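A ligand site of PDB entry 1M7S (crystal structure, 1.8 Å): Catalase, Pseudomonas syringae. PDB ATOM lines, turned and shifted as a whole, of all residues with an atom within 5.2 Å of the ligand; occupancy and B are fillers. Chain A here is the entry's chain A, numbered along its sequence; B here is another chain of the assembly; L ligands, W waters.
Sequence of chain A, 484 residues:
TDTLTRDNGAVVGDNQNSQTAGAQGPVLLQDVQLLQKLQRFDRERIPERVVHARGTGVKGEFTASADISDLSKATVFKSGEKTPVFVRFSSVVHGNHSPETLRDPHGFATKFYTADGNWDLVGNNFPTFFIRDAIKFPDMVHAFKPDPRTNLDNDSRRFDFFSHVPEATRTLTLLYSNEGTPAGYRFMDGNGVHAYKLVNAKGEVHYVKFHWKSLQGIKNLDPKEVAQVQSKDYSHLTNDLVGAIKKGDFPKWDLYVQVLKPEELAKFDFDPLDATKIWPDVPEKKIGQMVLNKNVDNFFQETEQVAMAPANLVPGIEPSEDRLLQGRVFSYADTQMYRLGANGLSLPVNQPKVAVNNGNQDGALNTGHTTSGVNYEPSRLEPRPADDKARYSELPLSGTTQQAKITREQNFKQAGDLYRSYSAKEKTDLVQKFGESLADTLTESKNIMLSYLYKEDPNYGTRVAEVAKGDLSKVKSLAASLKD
A ring nitrogen (NE2) of His 52 sits close to a nitrogen (N1) of the ligand, 3.5 Å away. Merely in contact with the ligand: Gly 123 (3.2 Å), Arg 328 (3.2 Å), Ser 331 (3.3 Å), Thr 335 (3.3 Å), Asn 124 (3.4 Å), His 194 (3.4 Å), Phe 137 (3.4 Å), Leu 324 (3.4 Å), Gly 107 (3.5 Å), Val 193 (3.5 Å), Val 51 (3.5 Å), Val 122 (3.6 Å), Gly 327 (3.6 Å), Phe 129 (3.7 Å), Met 308 (3.7 Å), Asp 42 of chain B (3.7 Å), Val 50 (3.7 Å), Ala 134 (3.7 Å), Phe 108 (3.9 Å), Leu 38 of chain B (3.9 Å) and Ala 109 (3.98 Å). The nearest printed residue that does not touch the ligand is Ser 90 (4.3 Å).
An oxygen (O1) of the ligand is in salt-bridge range of the guanidinium group (NE) of Arg 49 (2.9 Å). An oxygen (O4) of the ligand lies within salt-bridge range of the guanidinium group (NE) of Arg 339, at 2.8 Å. An iron atom (FE1) of the ligand is bound by the side-chain hydroxyl (OH) of Tyr 332 (2.0 Å). An oxygen (O3) of the ligand sits at hydrogen-bond distance from the side-chain amide nitrogen (NE2) of Gln 336 (2.8 Å). The guanidinium group of Arg 88 lies within salt-bridge range of an oxygen (O2) of the ligand, at 2.7 Å.
The backbone NH (N) of Asn 191 sits at hydrogen-bond distance from the backbone carbonyl oxygen (O) of Asn 124. The guanidinium group (NH2) of Arg 88 is in hydrogen-bond range of the backbone carbonyl oxygen (O) of His 52, at 3.0 Å. The backbone carbonyl oxygen (O) of Val 122 sits at hydrogen-bond distance from the guanidinium group (NH2) of Arg 328, at 3.1 Å. The side-chain hydroxyl (OH) of Tyr 332 lies close to the guanidinium group (NH2) of Arg 328, 2.6 Å away. A ring nitrogen (ND1) of His 52 is in hydrogen-bond range of the side-chain hydroxyl of Ser 90. The backbone carbonyl oxygen (O) of Gly 123 is in hydrogen-bond range of the backbone NH (N) of Phe 108 (2.9 Å). O of Ser 90 sits at hydrogen-bond distance from N of Gly 107, 2.8 Å away. NH1 of Arg 339 is in hydrogen-bond range of O of Val 306.
Water W1 lies within hydrogen-bond range of O1 of the ligand (2.6 Å), N of Met 308 (2.8 Å), O of Val 306 (3.3 Å) and NE2 of Gln 336 (3.4 Å). Water W3 lies within hydrogen-bond range of an oxygen (O4) of the ligand (2.7 Å), the side-chain hydroxyl (OG1) of Thr 335 (2.7 Å) and the backbone NH (N) of Val 50 (3.0 Å).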
ATOM      1  N   ARG A  49       9.948   7.528 -19.218  1.00  0.00           N
ATOM      2  CA  ARG A  49       8.582   7.289 -18.770  1.00  0.00           C
ATOM      3  C   ARG A  49       8.569   7.429 -17.220  1.00  0.00           C
ATOM      4  O   ARG A  49       9.521   7.016 -16.547  1.00  0.00           O
ATOM      5  CB  ARG A  49       8.065   5.924 -19.144  1.00  0.00           C
ATOM      6  CG  ARG A  49       7.889   5.692 -20.682  1.00  0.00           C
ATOM      7  CD  ARG A  49       7.890   4.203 -20.949  1.00  0.00           C
ATOM      8  NE  ARG A  49       7.533   3.939 -22.394  1.00  0.00           N
ATOM      9  CZ  ARG A  49       8.346   4.256 -23.380  1.00  0.00           C
ATOM     10  NH1 ARG A  49       9.576   4.762 -23.226  1.00  0.00           N
ATOM     11  NH2 ARG A  49       7.886   3.976 -24.606  1.00  0.00           N
ATOM     12  N   VAL A  50       7.490   8.020 -16.690  1.00  0.00           N
ATOM     13  CA  VAL A  50       7.374   8.267 -15.238  1.00  0.00           C
ATOM     14  C   VAL A  50       7.334   6.950 -14.488  1.00  0.00           C
ATOM     15  O   VAL A  50       7.794   6.878 -13.342  1.00  0.00           O
ATOM     16  CB  VAL A  50       6.164   9.176 -14.972  1.00  0.00           C
ATOM     17  CG1 VAL A  50       4.825   8.448 -15.192  1.00  0.00           C
ATOM     18  CG2 VAL A  50       6.156   9.682 -13.527  1.00  0.00           C
ATOM     19  N   VAL A  51       6.858   5.875 -15.115  1.00  0.00           N
ATOM     20  CA  VAL A  51       6.922   4.533 -14.620  1.00  0.00           C
ATOM     21  C   VAL A  51       7.235   3.643 -15.903  1.00  0.00           C
ATOM     22  O   VAL A  51       6.920   4.133 -16.986  1.00  0.00           O
ATOM     23  CB  VAL A  51       5.728   3.936 -13.871  1.00  0.00           C
ATOM     24  CG1 VAL A  51       5.547   4.578 -12.469  1.00  0.00           C
ATOM     25  CG2 VAL A  51       4.430   4.134 -14.647  1.00  0.00           C
ATOM     26  N   HIS A  52       7.717   2.448 -15.629  1.00  0.00           N
ATOM     27  CA  HIS A  52       8.100   1.522 -16.738  1.00  0.00           C
ATOM     28  C   HIS A  52       9.119   2.192 -17.663  1.00  0.00           C
ATOM     29  O   HIS A  52       9.231   1.926 -18.853  1.00  0.00           O
ATOM     30  CB  HIS A  52       6.847   1.100 -17.509  1.00  0.00           C
ATOM     31  CG  HIS A  52       5.826   0.313 -16.718  1.00  0.00           C
ATOM     32  ND1 HIS A  52       5.732  -1.031 -16.862  1.00  0.00           N
ATOM     33  CD2 HIS A  52       4.862   0.662 -15.832  1.00  0.00           C
ATOM     34  CE1 HIS A  52       4.744  -1.504 -16.076  1.00  0.00           C
ATOM     35  NE2 HIS A  52       4.210  -0.456 -15.443  1.00  0.00           N
ATOM     36  N   ARG A  88       6.164  -3.721 -26.060  1.00  0.00           N
ATOM     37  CA  ARG A  88       7.255  -3.179 -25.213  1.00  0.00           C
ATOM     38  C   ARG A  88       7.064  -3.927 -23.855  1.00  0.00           C
ATOM     39  O   ARG A  88       5.967  -3.907 -23.269  1.00  0.00           O
ATOM     40  CB  ARG A  88       7.144  -1.659 -24.992  1.00  0.00           C
ATOM     41  CG  ARG A  88       8.424  -1.146 -24.227  1.00  0.00           C
ATOM     42  CD  ARG A  88       8.447   0.392 -24.446  1.00  0.00           C
ATOM     43  NE  ARG A  88       9.437   0.965 -23.488  1.00  0.00           N
ATOM     44  CZ  ARG A  88       9.310   1.102 -22.184  1.00  0.00           C
ATOM     45  NH1 ARG A  88       8.264   0.756 -21.450  1.00  0.00           N
ATOM     46  NH2 ARG A  88      10.395   1.665 -21.585  1.00  0.00           N
ATOM     47  N   PHE A  89       8.159  -4.566 -23.404  1.00  0.00           N
ATOM     48  CA  PHE A  89       8.188  -5.269 -22.137  1.00  0.00           C
ATOM     49  C   PHE A  89       8.916  -4.315 -21.155  1.00  0.00           C
ATOM     50  O   PHE A  89       9.754  -3.590 -21.671  1.00  0.00           O
ATOM     51  CB  PHE A  89       9.018  -6.570 -22.207  1.00  0.00           C
ATOM     52  CG  PHE A  89       8.280  -7.686 -22.943  1.00  0.00           C
ATOM     53  CD1 PHE A  89       7.200  -8.321 -22.393  1.00  0.00           C
ATOM     54  CD2 PHE A  89       8.730  -8.070 -24.206  1.00  0.00           C
ATOM     55  CE1 PHE A  89       6.541  -9.332 -23.076  1.00  0.00           C
ATOM     56  CE2 PHE A  89       8.105  -9.075 -24.916  1.00  0.00           C
ATOM     57  CZ  PHE A  89       7.003  -9.714 -24.331  1.00  0.00           C
ATOM     58  N   SER A  90       8.669  -4.414 -19.855  1.00  0.00           N
ATOM     59  CA  SER A  90       9.405  -3.450 -18.993  1.00  0.00           C
ATOM     60  C   SER A  90       9.376  -3.825 -17.536  1.00  0.00           C
ATOM     61  O   SER A  90       8.602  -4.716 -17.167  1.00  0.00           O
ATOM     62  CB  SER A  90       8.672  -2.098 -19.100  1.00  0.00           C
ATOM     63  OG  SER A  90       7.271  -2.236 -18.879  1.00  0.00           O
ATOM     64  N   GLY A 107       5.815  -5.025 -17.119  1.00  0.00           N
ATOM     65  CA  GLY A 107       4.838  -4.597 -18.141  1.00  0.00           C
ATOM     66  C   GLY A 107       4.904  -5.516 -19.360  1.00  0.00           C
ATOM     67  O   GLY A 107       5.982  -6.002 -19.722  1.00  0.00           O
ATOM     68  N   PHE A 108       3.795  -5.577 -20.055  1.00  0.00           N
ATOM     69  CA  PHE A 108       3.623  -6.357 -21.311  1.00  0.00           C
ATOM     70  C   PHE A 108       2.594  -5.615 -22.124  1.00  0.00           C
ATOM     71  O   PHE A 108       1.392  -5.740 -21.928  1.00  0.00           O
ATOM     72  CB  PHE A 108       3.158  -7.757 -20.924  1.00  0.00           C
ATOM     73  CG  PHE A 108       3.102  -8.800 -22.021  1.00  0.00           C
ATOM     74  CD1 PHE A 108       3.117 -10.135 -21.675  1.00  0.00           C
ATOM     75  CD2 PHE A 108       3.016  -8.479 -23.381  1.00  0.00           C
ATOM     76  CE1 PHE A 108       3.070 -11.154 -22.618  1.00  0.00           C
ATOM     77  CE2 PHE A 108       2.986  -9.479 -24.342  1.00  0.00           C
ATOM     78  CZ  PHE A 108       3.010 -10.826 -23.940  1.00  0.00           C
ATOM     79  N   ALA A 109       3.014  -4.585 -22.874  1.00  0.00           N
ATOM     80  CA  ALA A 109       2.165  -3.681 -23.630  1.00  0.00           C
ATOM     81  C   ALA A 109       2.216  -4.024 -25.134  1.00  0.00           C
ATOM     82  O   ALA A 109       3.286  -4.023 -25.774  1.00  0.00           O
ATOM     83  CB  ALA A 109       2.609  -2.239 -23.380  1.00  0.00           C
ATOM     84  N   VAL A 122      -2.478  -2.593 -22.811  1.00  0.00           N
ATOM     85  CA  VAL A 122      -1.343  -2.290 -21.911  1.00  0.00           C
ATOM     86  C   VAL A 122      -1.466  -3.102 -20.620  1.00  0.00           C
ATOM     87  O   VAL A 122      -2.295  -2.737 -19.766  1.00  0.00           O
ATOM     88  CB  VAL A 122      -1.367  -0.783 -21.598  1.00  0.00           C
ATOM     89  CG1 VAL A 122      -0.092  -0.381 -20.859  1.00  0.00           C
ATOM     90  CG2 VAL A 122      -1.487  -0.003 -22.911  1.00  0.00           C
ATOM     91  N   GLY A 123      -0.759  -4.241 -20.607  1.00  0.00           N
ATOM     92  CA  GLY A 123      -0.949  -5.140 -19.460  1.00  0.00           C
ATOM     93  C   GLY A 123       0.336  -5.324 -18.638  1.00  0.00           C
ATOM     94  O   GLY A 123       1.304  -4.671 -18.828  1.00  0.00           O
ATOM     95  N   ASN A 124       0.359  -6.300 -17.760  1.00  0.00           N
ATOM     96  CA  ASN A 124       1.406  -6.695 -16.882  1.00  0.00           C
ATOM     97  C   ASN A 124       1.421  -8.211 -16.752  1.00  0.00           C
ATOM     98  O   ASN A 124       0.416  -8.883 -17.046  1.00  0.00           O
ATOM     99  CB  ASN A 124       1.164  -6.126 -15.451  1.00  0.00           C
ATOM    100  CG  ASN A 124       1.747  -4.767 -15.206  1.00  0.00           C
ATOM    101  OD1 ASN A 124       2.498  -4.164 -15.973  1.00  0.00           O
ATOM    102  ND2 ASN A 124       1.396  -4.130 -14.079  1.00  0.00           N
ATOM    103  N   PHE A 129      -3.685  -5.783  -9.490  1.00  0.00           N
ATOM    104  CA  PHE A 129      -2.858  -4.606  -9.157  1.00  0.00           C
ATOM    105  C   PHE A 129      -2.970  -4.304  -7.668  1.00  0.00           C
ATOM    106  O   PHE A 129      -3.744  -4.981  -6.957  1.00  0.00           O
ATOM    107  CB  PHE A 129      -3.352  -3.413  -9.984  1.00  0.00           C
ATOM    108  CG  PHE A 129      -2.238  -2.414 -10.151  1.00  0.00           C
ATOM    109  CD1 PHE A 129      -2.381  -1.114  -9.651  1.00  0.00           C
ATOM    110  CD2 PHE A 129      -1.069  -2.774 -10.800  1.00  0.00           C
ATOM    111  CE1 PHE A 129      -1.344  -0.221  -9.822  1.00  0.00           C
ATOM    112  CE2 PHE A 129      -0.030  -1.875 -10.963  1.00  0.00           C
ATOM    113  CZ  PHE A 129      -0.178  -0.590 -10.452  1.00  0.00           C
ATOM    114  N   ALA A 134      -7.637   4.948  -9.437  1.00  0.00           N
ATOM    115  CA  ALA A 134      -6.520   5.724  -9.993  1.00  0.00           C
ATOM    116  C   ALA A 134      -6.198   6.981  -9.223  1.00  0.00           C
ATOM    117  O   ALA A 134      -5.040   7.425  -9.302  1.00  0.00           O
ATOM    118  CB  ALA A 134      -6.788   6.041 -11.463  1.00  0.00           C
ATOM    119  N   PHE A 137      -2.916   6.367  -7.555  1.00  0.00           N
ATOM    120  CA  PHE A 137      -1.740   5.936  -8.309  1.00  0.00           C
ATOM    121  C   PHE A 137      -0.482   6.749  -8.018  1.00  0.00           C
ATOM    122  O   PHE A 137       0.550   6.165  -7.731  1.00  0.00           O
ATOM    123  CB  PHE A 137      -2.025   5.858  -9.837  1.00  0.00           C
ATOM    124  CG  PHE A 137      -0.898   5.207 -10.592  1.00  0.00           C
ATOM    125  CD1 PHE A 137      -0.714   3.845 -10.506  1.00  0.00           C
ATOM    126  CD2 PHE A 137      -0.074   5.969 -11.425  1.00  0.00           C
ATOM    127  CE1 PHE A 137       0.315   3.237 -11.219  1.00  0.00           C
ATOM    128  CE2 PHE A 137       0.952   5.353 -12.132  1.00  0.00           C
ATOM    129  CZ  PHE A 137       1.130   3.978 -12.049  1.00  0.00           C
ATOM    130  N   ASN A 191      -1.335 -10.133 -18.747  1.00  0.00           N
ATOM    131  CA  ASN A 191      -2.739  -9.983 -18.379  1.00  0.00           C
ATOM    132  C   ASN A 191      -3.180  -8.544 -18.591  1.00  0.00           C
ATOM    133  O   ASN A 191      -2.424  -7.638 -18.268  1.00  0.00           O
ATOM    134  CB  ASN A 191      -2.958 -10.350 -16.901  1.00  0.00           C
ATOM    135  CG  ASN A 191      -2.775 -11.843 -16.644  1.00  0.00           C
ATOM    136  OD1 ASN A 191      -3.642 -12.629 -16.933  1.00  0.00           O
ATOM    137  ND2 ASN A 191      -1.608 -12.265 -16.135  1.00  0.00           N
ATOM    138  N   GLY A 192      -4.438  -8.304 -18.987  1.00  0.00           N
ATOM    139  CA  GLY A 192      -4.977  -6.952 -19.121  1.00  0.00           C
ATOM    140  C   GLY A 192      -5.271  -6.340 -17.762  1.00  0.00           C
ATOM    141  O   GLY A 192      -5.316  -5.112 -17.681  1.00  0.00           O
ATOM    142  N   VAL A 193      -5.400  -7.181 -16.748  1.00  0.00           N
ATOM    143  CA  VAL A 193      -5.797  -6.866 -15.396  1.00  0.00           C
ATOM    144  C   VAL A 193      -7.280  -6.504 -15.301  1.00  0.00           C
ATOM    145  O   VAL A 193      -8.051  -7.267 -14.683  1.00  0.00           O
ATOM    146  CB  VAL A 193      -4.914  -5.810 -14.718  1.00  0.00           C
ATOM    147  CG1 VAL A 193      -5.348  -5.594 -13.289  1.00  0.00           C
ATOM    148  CG2 VAL A 193      -3.452  -6.313 -14.713  1.00  0.00           C
ATOM    149  N   HIS A 194      -7.691  -5.429 -15.917  1.00  0.00           N
ATOM    150  CA  HIS A 194      -9.075  -5.010 -15.855  1.00  0.00           C
ATOM    151  C   HIS A 194      -9.979  -5.820 -16.787  1.00  0.00           C
ATOM    152  O   HIS A 194      -9.493  -6.309 -17.794  1.00  0.00           O
ATOM    153  CB  HIS A 194      -9.196  -3.581 -16.452  1.00  0.00           C
ATOM    154  CG  HIS A 194      -8.120  -2.655 -16.001  1.00  0.00           C
ATOM    155  ND1 HIS A 194      -8.064  -2.238 -14.692  1.00  0.00           N
ATOM    156  CD2 HIS A 194      -7.056  -2.096 -16.657  1.00  0.00           C
ATOM    157  CE1 HIS A 194      -7.005  -1.440 -14.549  1.00  0.00           C
ATOM    158  NE2 HIS A 194      -6.407  -1.329 -15.699  1.00  0.00           N
ATOM    159  N   VAL A 306       7.729   4.830 -28.559  1.00  0.00           N
ATOM    160  CA  VAL A 306       6.402   4.248 -28.705  1.00  0.00           C
ATOM    161  C   VAL A 306       5.492   4.773 -27.618  1.00  0.00           C
ATOM    162  O   VAL A 306       5.880   4.995 -26.466  1.00  0.00           O
ATOM    163  CB  VAL A 306       6.484   2.714 -28.771  1.00  0.00           C
ATOM    164  CG1 VAL A 306       6.821   2.061 -27.428  1.00  0.00           C
ATOM    165  CG2 VAL A 306       5.213   2.125 -29.391  1.00  0.00           C
ATOM    166  N   ALA A 307       4.229   5.021 -27.956  1.00  0.00           N
ATOM    167  CA  ALA A 307       3.223   5.606 -27.074  1.00  0.00           C
ATOM    168  C   ALA A 307       2.091   4.586 -26.875  1.00  0.00           C
ATOM    169  O   ALA A 307       1.284   4.393 -27.782  1.00  0.00           O
ATOM    170  CB  ALA A 307       2.707   6.898 -27.698  1.00  0.00           C
ATOM    171  N   MET A 308       2.184   3.822 -25.774  1.00  0.00           N
ATOM    172  CA  MET A 308       1.143   2.825 -25.484  1.00  0.00           C
ATOM    173  C   MET A 308       0.068   3.483 -24.627  1.00  0.00           C
ATOM    174  O   MET A 308       0.455   4.114 -23.630  1.00  0.00           O
ATOM    175  CB  MET A 308       1.753   1.678 -24.663  1.00  0.00           C
ATOM    176  CG  MET A 308       2.913   0.912 -25.329  1.00  0.00           C
ATOM    177  SD  MET A 308       2.177  -0.060 -26.694  1.00  0.00           S
ATOM    178  CE  MET A 308       3.634  -0.998 -27.185  1.00  0.00           C
ATOM    179  N   LEU A 324      -9.729   2.015 -11.599  1.00  0.00           N
ATOM    180  CA  LEU A 324      -8.321   2.174 -11.873  1.00  0.00           C
ATOM    181  C   LEU A 324      -8.151   2.404 -13.382  1.00  0.00           C
ATOM    182  O   LEU A 324      -7.385   3.260 -13.849  1.00  0.00           O
ATOM    183  CB  LEU A 324      -7.620   0.859 -11.445  1.00  0.00           C
ATOM    184  CG  LEU A 324      -6.099   0.979 -11.359  1.00  0.00           C
ATOM    185  CD1 LEU A 324      -5.706   1.975 -10.280  1.00  0.00           C
ATOM    186  CD2 LEU A 324      -5.510  -0.399 -11.100  1.00  0.00           C
ATOM    187  N   GLY A 327      -9.005   6.007 -14.796  1.00  0.00           N
ATOM    188  CA  GLY A 327      -7.860   6.944 -14.722  1.00  0.00           C
ATOM    189  C   GLY A 327      -6.813   6.717 -15.802  1.00  0.00           C
ATOM    190  O   GLY A 327      -6.208   7.690 -16.316  1.00  0.00           O
ATOM    191  N   ARG A 328      -6.601   5.463 -16.193  1.00  0.00           N
ATOM    192  CA  ARG A 328      -5.592   5.108 -17.201  1.00  0.00           C
ATOM    193  C   ARG A 328      -6.025   5.589 -18.574  1.00  0.00           C
ATOM    194  O   ARG A 328      -5.164   5.991 -19.359  1.00  0.00           O
ATOM    195  CB  ARG A 328      -5.332   3.607 -17.224  1.00  0.00           C
ATOM    196  CG  ARG A 328      -4.837   3.023 -15.903  1.00  0.00           C
ATOM    197  CD  ARG A 328      -4.642   1.490 -16.083  1.00  0.00           C
ATOM    198  NE  ARG A 328      -3.467   1.303 -16.933  1.00  0.00           N
ATOM    199  CZ  ARG A 328      -3.339   0.179 -17.654  1.00  0.00           C
ATOM    200  NH1 ARG A 328      -4.309  -0.747 -17.595  1.00  0.00           N
ATOM    201  NH2 ARG A 328      -2.263  -0.001 -18.389  1.00  0.00           N
ATOM    202  N   SER A 331      -4.551   9.172 -18.268  1.00  0.00           N
ATOM    203  CA  SER A 331      -3.123   9.428 -17.967  1.00  0.00           C
ATOM    204  C   SER A 331      -2.059   9.131 -18.994  1.00  0.00           C
ATOM    205  O   SER A 331      -1.014   9.823 -19.062  1.00  0.00           O
ATOM    206  CB  SER A 331      -2.824   8.612 -16.665  1.00  0.00           C
ATOM    207  OG  SER A 331      -1.450   8.847 -16.383  1.00  0.00           O
ATOM    208  N   TYR A 332      -2.253   8.078 -19.779  1.00  0.00           N
ATOM    209  CA  TYR A 332      -1.137   7.738 -20.734  1.00  0.00           C
ATOM    210  C   TYR A 332      -1.164   8.763 -21.841  1.00  0.00           C
ATOM    211  O   TYR A 332      -0.147   9.322 -22.196  1.00  0.00           O
ATOM    212  CB  TYR A 332      -1.376   6.339 -21.290  1.00  0.00           C
ATOM    213  CG  TYR A 332      -1.234   5.213 -20.291  1.00  0.00           C
ATOM    214  CD1 TYR A 332      -0.200   4.285 -20.462  1.00  0.00           C
ATOM    215  CD2 TYR A 332      -2.076   5.121 -19.183  1.00  0.00           C
ATOM    216  CE1 TYR A 332      -0.091   3.204 -19.593  1.00  0.00           C
ATOM    217  CE2 TYR A 332      -1.927   4.062 -18.317  1.00  0.00           C
ATOM    218  CZ  TYR A 332      -0.962   3.103 -18.544  1.00  0.00           C
ATOM    219  OH  TYR A 332      -0.835   2.061 -17.632  1.00  0.00           O
ATOM    220  N   THR A 335       0.416  11.968 -20.356  1.00  0.00           N
ATOM    221  CA  THR A 335       1.897  12.006 -20.191  1.00  0.00           C
ATOM    222  C   THR A 335       2.594  11.969 -21.551  1.00  0.00           C
ATOM    223  O   THR A 335       3.703  12.485 -21.698  1.00  0.00           O
ATOM    224  CB  THR A 335       2.352  10.884 -19.224  1.00  0.00           C
ATOM    225  OG1 THR A 335       3.722  11.118 -18.827  1.00  0.00           O
ATOM    226  CG2 THR A 335       2.414   9.528 -19.971  1.00  0.00           C
ATOM    227  N   GLN A 336       1.998  11.391 -22.599  1.00  0.00           N
ATOM    228  CA  GLN A 336       2.650  11.317 -23.909  1.00  0.00           C
ATOM    229  C   GLN A 336       2.649  12.679 -24.587  1.00  0.00           C
ATOM    230  O   GLN A 336       3.528  13.069 -25.345  1.00  0.00           O
ATOM    231  CB  GLN A 336       1.995  10.207 -24.751  1.00  0.00           C
ATOM    232  CG  GLN A 336       2.427   8.809 -24.253  1.00  0.00           C
ATOM    233  CD  GLN A 336       1.432   7.673 -24.408  1.00  0.00           C
ATOM    234  OE1 GLN A 336       0.372   7.747 -25.059  1.00  0.00           O
ATOM    235  NE2 GLN A 336       1.754   6.562 -23.764  1.00  0.00           N
ATOM    236  N   ARG A 339       5.874  13.898 -22.710  1.00  0.00           N
ATOM    237  CA  ARG A 339       7.083  13.115 -22.984  1.00  0.00           C
ATOM    238  C   ARG A 339       7.475  13.143 -24.459  1.00  0.00           C
ATOM    239  O   ARG A 339       8.659  13.194 -24.811  1.00  0.00           O
ATOM    240  CB  ARG A 339       6.838  11.621 -22.596  1.00  0.00           C
ATOM    241  CG  ARG A 339       8.112  10.777 -22.628  1.00  0.00           C
ATOM    242  CD  ARG A 339       7.869   9.427 -21.951  1.00  0.00           C
ATOM    243  NE  ARG A 339       6.909   8.557 -22.663  1.00  0.00           N
ATOM    244  CZ  ARG A 339       7.142   7.866 -23.764  1.00  0.00           C
ATOM    245  NH1 ARG A 339       6.164   7.075 -24.249  1.00  0.00           N
ATOM    246  NH2 ARG A 339       8.298   7.842 -24.430  1.00  0.00           N
ATOM    247  N   LEU B  38      -3.052  13.687 -11.401  1.00  0.00           N
ATOM    248  CA  LEU B  38      -2.498  12.968 -12.553  1.00  0.00           C
ATOM    249  C   LEU B  38      -1.701  13.862 -13.501  1.00  0.00           C
ATOM    250  O   LEU B  38      -0.643  13.441 -13.924  1.00  0.00           O
ATOM    251  CB  LEU B  38      -3.618  12.207 -13.271  1.00  0.00           C
ATOM    252  CG  LEU B  38      -4.255  11.061 -12.435  1.00  0.00           C
ATOM    253  CD1 LEU B  38      -5.398  10.474 -13.296  1.00  0.00           C
ATOM    254  CD2 LEU B  38      -3.228  10.014 -12.066  1.00  0.00           C
ATOM    255  N   PHE B  41       1.704  14.345 -11.823  1.00  0.00           N
ATOM    256  CA  PHE B  41       2.423  13.083 -11.844  1.00  0.00           C
ATOM    257  C   PHE B  41       3.014  12.765 -13.209  1.00  0.00           C
ATOM    258  O   PHE B  41       4.172  12.399 -13.429  1.00  0.00           O
ATOM    259  CB  PHE B  41       1.416  11.949 -11.476  1.00  0.00           C
ATOM    260  CG  PHE B  41       2.070  10.586 -11.522  1.00  0.00           C
ATOM    261  CD1 PHE B  41       2.957  10.184 -10.561  1.00  0.00           C
ATOM    262  CD2 PHE B  41       1.771   9.736 -12.590  1.00  0.00           C
ATOM    263  CE1 PHE B  41       3.586   8.923 -10.640  1.00  0.00           C
ATOM    264  CE2 PHE B  41       2.363   8.513 -12.656  1.00  0.00           C
ATOM    265  CZ  PHE B  41       3.280   8.079 -11.686  1.00  0.00           C
ATOM    266  N   ASP B  42       2.123  12.984 -14.222  1.00  0.00           N
ATOM    267  CA  ASP B  42       2.449  12.736 -15.606  1.00  0.00           C
ATOM    268  C   ASP B  42       3.584  13.653 -16.124  1.00  0.00           C
ATOM    269  O   ASP B  42       4.161  13.311 -17.170  1.00  0.00           O
ATOM    270  CB  ASP B  42       1.200  13.043 -16.508  1.00  0.00           C
ATOM    271  CG  ASP B  42       0.081  12.035 -16.371  1.00  0.00           C
ATOM    272  OD1 ASP B  42      -1.118  12.236 -16.773  1.00  0.00           O
ATOM    273  OD2 ASP B  42       0.393  10.968 -15.827  1.00  0.00           O
HETATM  274  C1  LIG L   1       3.130   2.995 -18.146  1.00  0.00           C
HETATM  275  C2  LIG L   1       0.789  -1.094 -17.039  1.00  0.00           C
HETATM  276  C3  LIG L   1      -1.792   1.304 -13.732  1.00  0.00           C
HETATM  277  C4  LIG L   1      -0.159   5.511 -15.536  1.00  0.00           C
HETATM  278  C5  LIG L   1       2.722   1.678 -18.117  1.00  0.00           C
HETATM  279  C6  LIG L   1       3.318   0.596 -18.934  1.00  0.00           C
HETATM  280  C7  LIG L   1       2.668  -0.533 -18.625  1.00  0.00           C
HETATM  281  C8  LIG L   1       1.684  -0.197 -17.613  1.00  0.00           C
HETATM  282  C9  LIG L   1       2.850  -1.937 -19.206  1.00  0.00           C
HETATM  283  C10 LIG L   1       4.444   0.860 -19.939  1.00  0.00           C
HETATM  284  C11 LIG L   1       3.989   0.941 -21.429  1.00  0.00           C
HETATM  285  C12 LIG L   1       5.246   1.009 -22.336  1.00  0.00           C
HETATM  286  O1  LIG L   1       5.391   2.110 -22.905  1.00  0.00           O
HETATM  287  O2  LIG L   1       5.862  -0.082 -22.373  1.00  0.00           O
HETATM  288  C13 LIG L   1      -0.132  -0.809 -16.077  1.00  0.00           C
HETATM  289  C14 LIG L   1      -1.116  -1.733 -15.531  1.00  0.00           C
HETATM  290  C15 LIG L   1      -1.828  -1.072 -14.598  1.00  0.00           C
HETATM  291  C16 LIG L   1      -1.316   0.274 -14.557  1.00  0.00           C
HETATM  292  C17 LIG L   1      -1.224  -3.200 -15.975  1.00  0.00           C
HETATM  293  C18 LIG L   1      -2.954  -1.533 -13.675  1.00  0.00           C
HETATM  294  C19 LIG L   1      -3.777  -2.524 -13.970  1.00  0.00           C
HETATM  295  C20 LIG L   1      -1.643   2.635 -14.020  1.00  0.00           C
HETATM  296  C21 LIG L   1      -2.488   3.681 -13.505  1.00  0.00           C
HETATM  297  C22 LIG L   1      -2.060   4.853 -14.017  1.00  0.00           C
HETATM  298  C23 LIG L   1      -0.894   4.538 -14.830  1.00  0.00           C
HETATM  299  C24 LIG L   1      -3.725   3.501 -12.580  1.00  0.00           C
HETATM  300  C25 LIG L   1      -2.580   6.284 -13.836  1.00  0.00           C
HETATM  301  C26 LIG L   1      -3.888   6.599 -13.769  1.00  0.00           C
HETATM  302  C27 LIG L   1       0.931   5.165 -16.342  1.00  0.00           C
HETATM  303  C28 LIG L   1       1.786   6.135 -17.011  1.00  0.00           C
HETATM  304  C29 LIG L   1       2.684   5.451 -17.731  1.00  0.00           C
HETATM  305  C30 LIG L   1       2.424   4.050 -17.535  1.00  0.00           C
HETATM  306  C31 LIG L   1       1.604   7.647 -16.835  1.00  0.00           C
HETATM  307  C32 LIG L   1       3.822   6.013 -18.637  1.00  0.00           C
HETATM  308  C33 LIG L   1       3.312   6.039 -20.121  1.00  0.00           C
HETATM  309  C34 LIG L   1       4.258   6.747 -21.084  1.00  0.00           C
HETATM  310  O3  LIG L   1       4.174   6.407 -22.309  1.00  0.00           O
HETATM  311  O4  LIG L   1       5.058   7.649 -20.711  1.00  0.00           O
HETATM  312  N1  LIG L   1       1.772   1.136 -17.299  1.00  0.00           N
HETATM  313  N2  LIG L   1      -0.295   0.429 -15.481  1.00  0.00           N
HETATM  314  N3  LIG L   1      -0.657   3.179 -14.801  1.00  0.00           N
HETATM  315  N4  LIG L   1       1.321   3.896 -16.733  1.00  0.00           N
HETATM  316 FE1  LIG L   1       0.493   2.170 -16.124  1.00  0.00          FE
HETATM  317  O   HOH W   1       4.148   4.187 -23.751  1.00  0.00           O
HETATM  318  O   HOH W   2       1.750   1.389 -14.097  1.00  0.00           O
HETATM  319  O   HOH W   3       5.813   9.357 -18.730  1.00  0.00           O
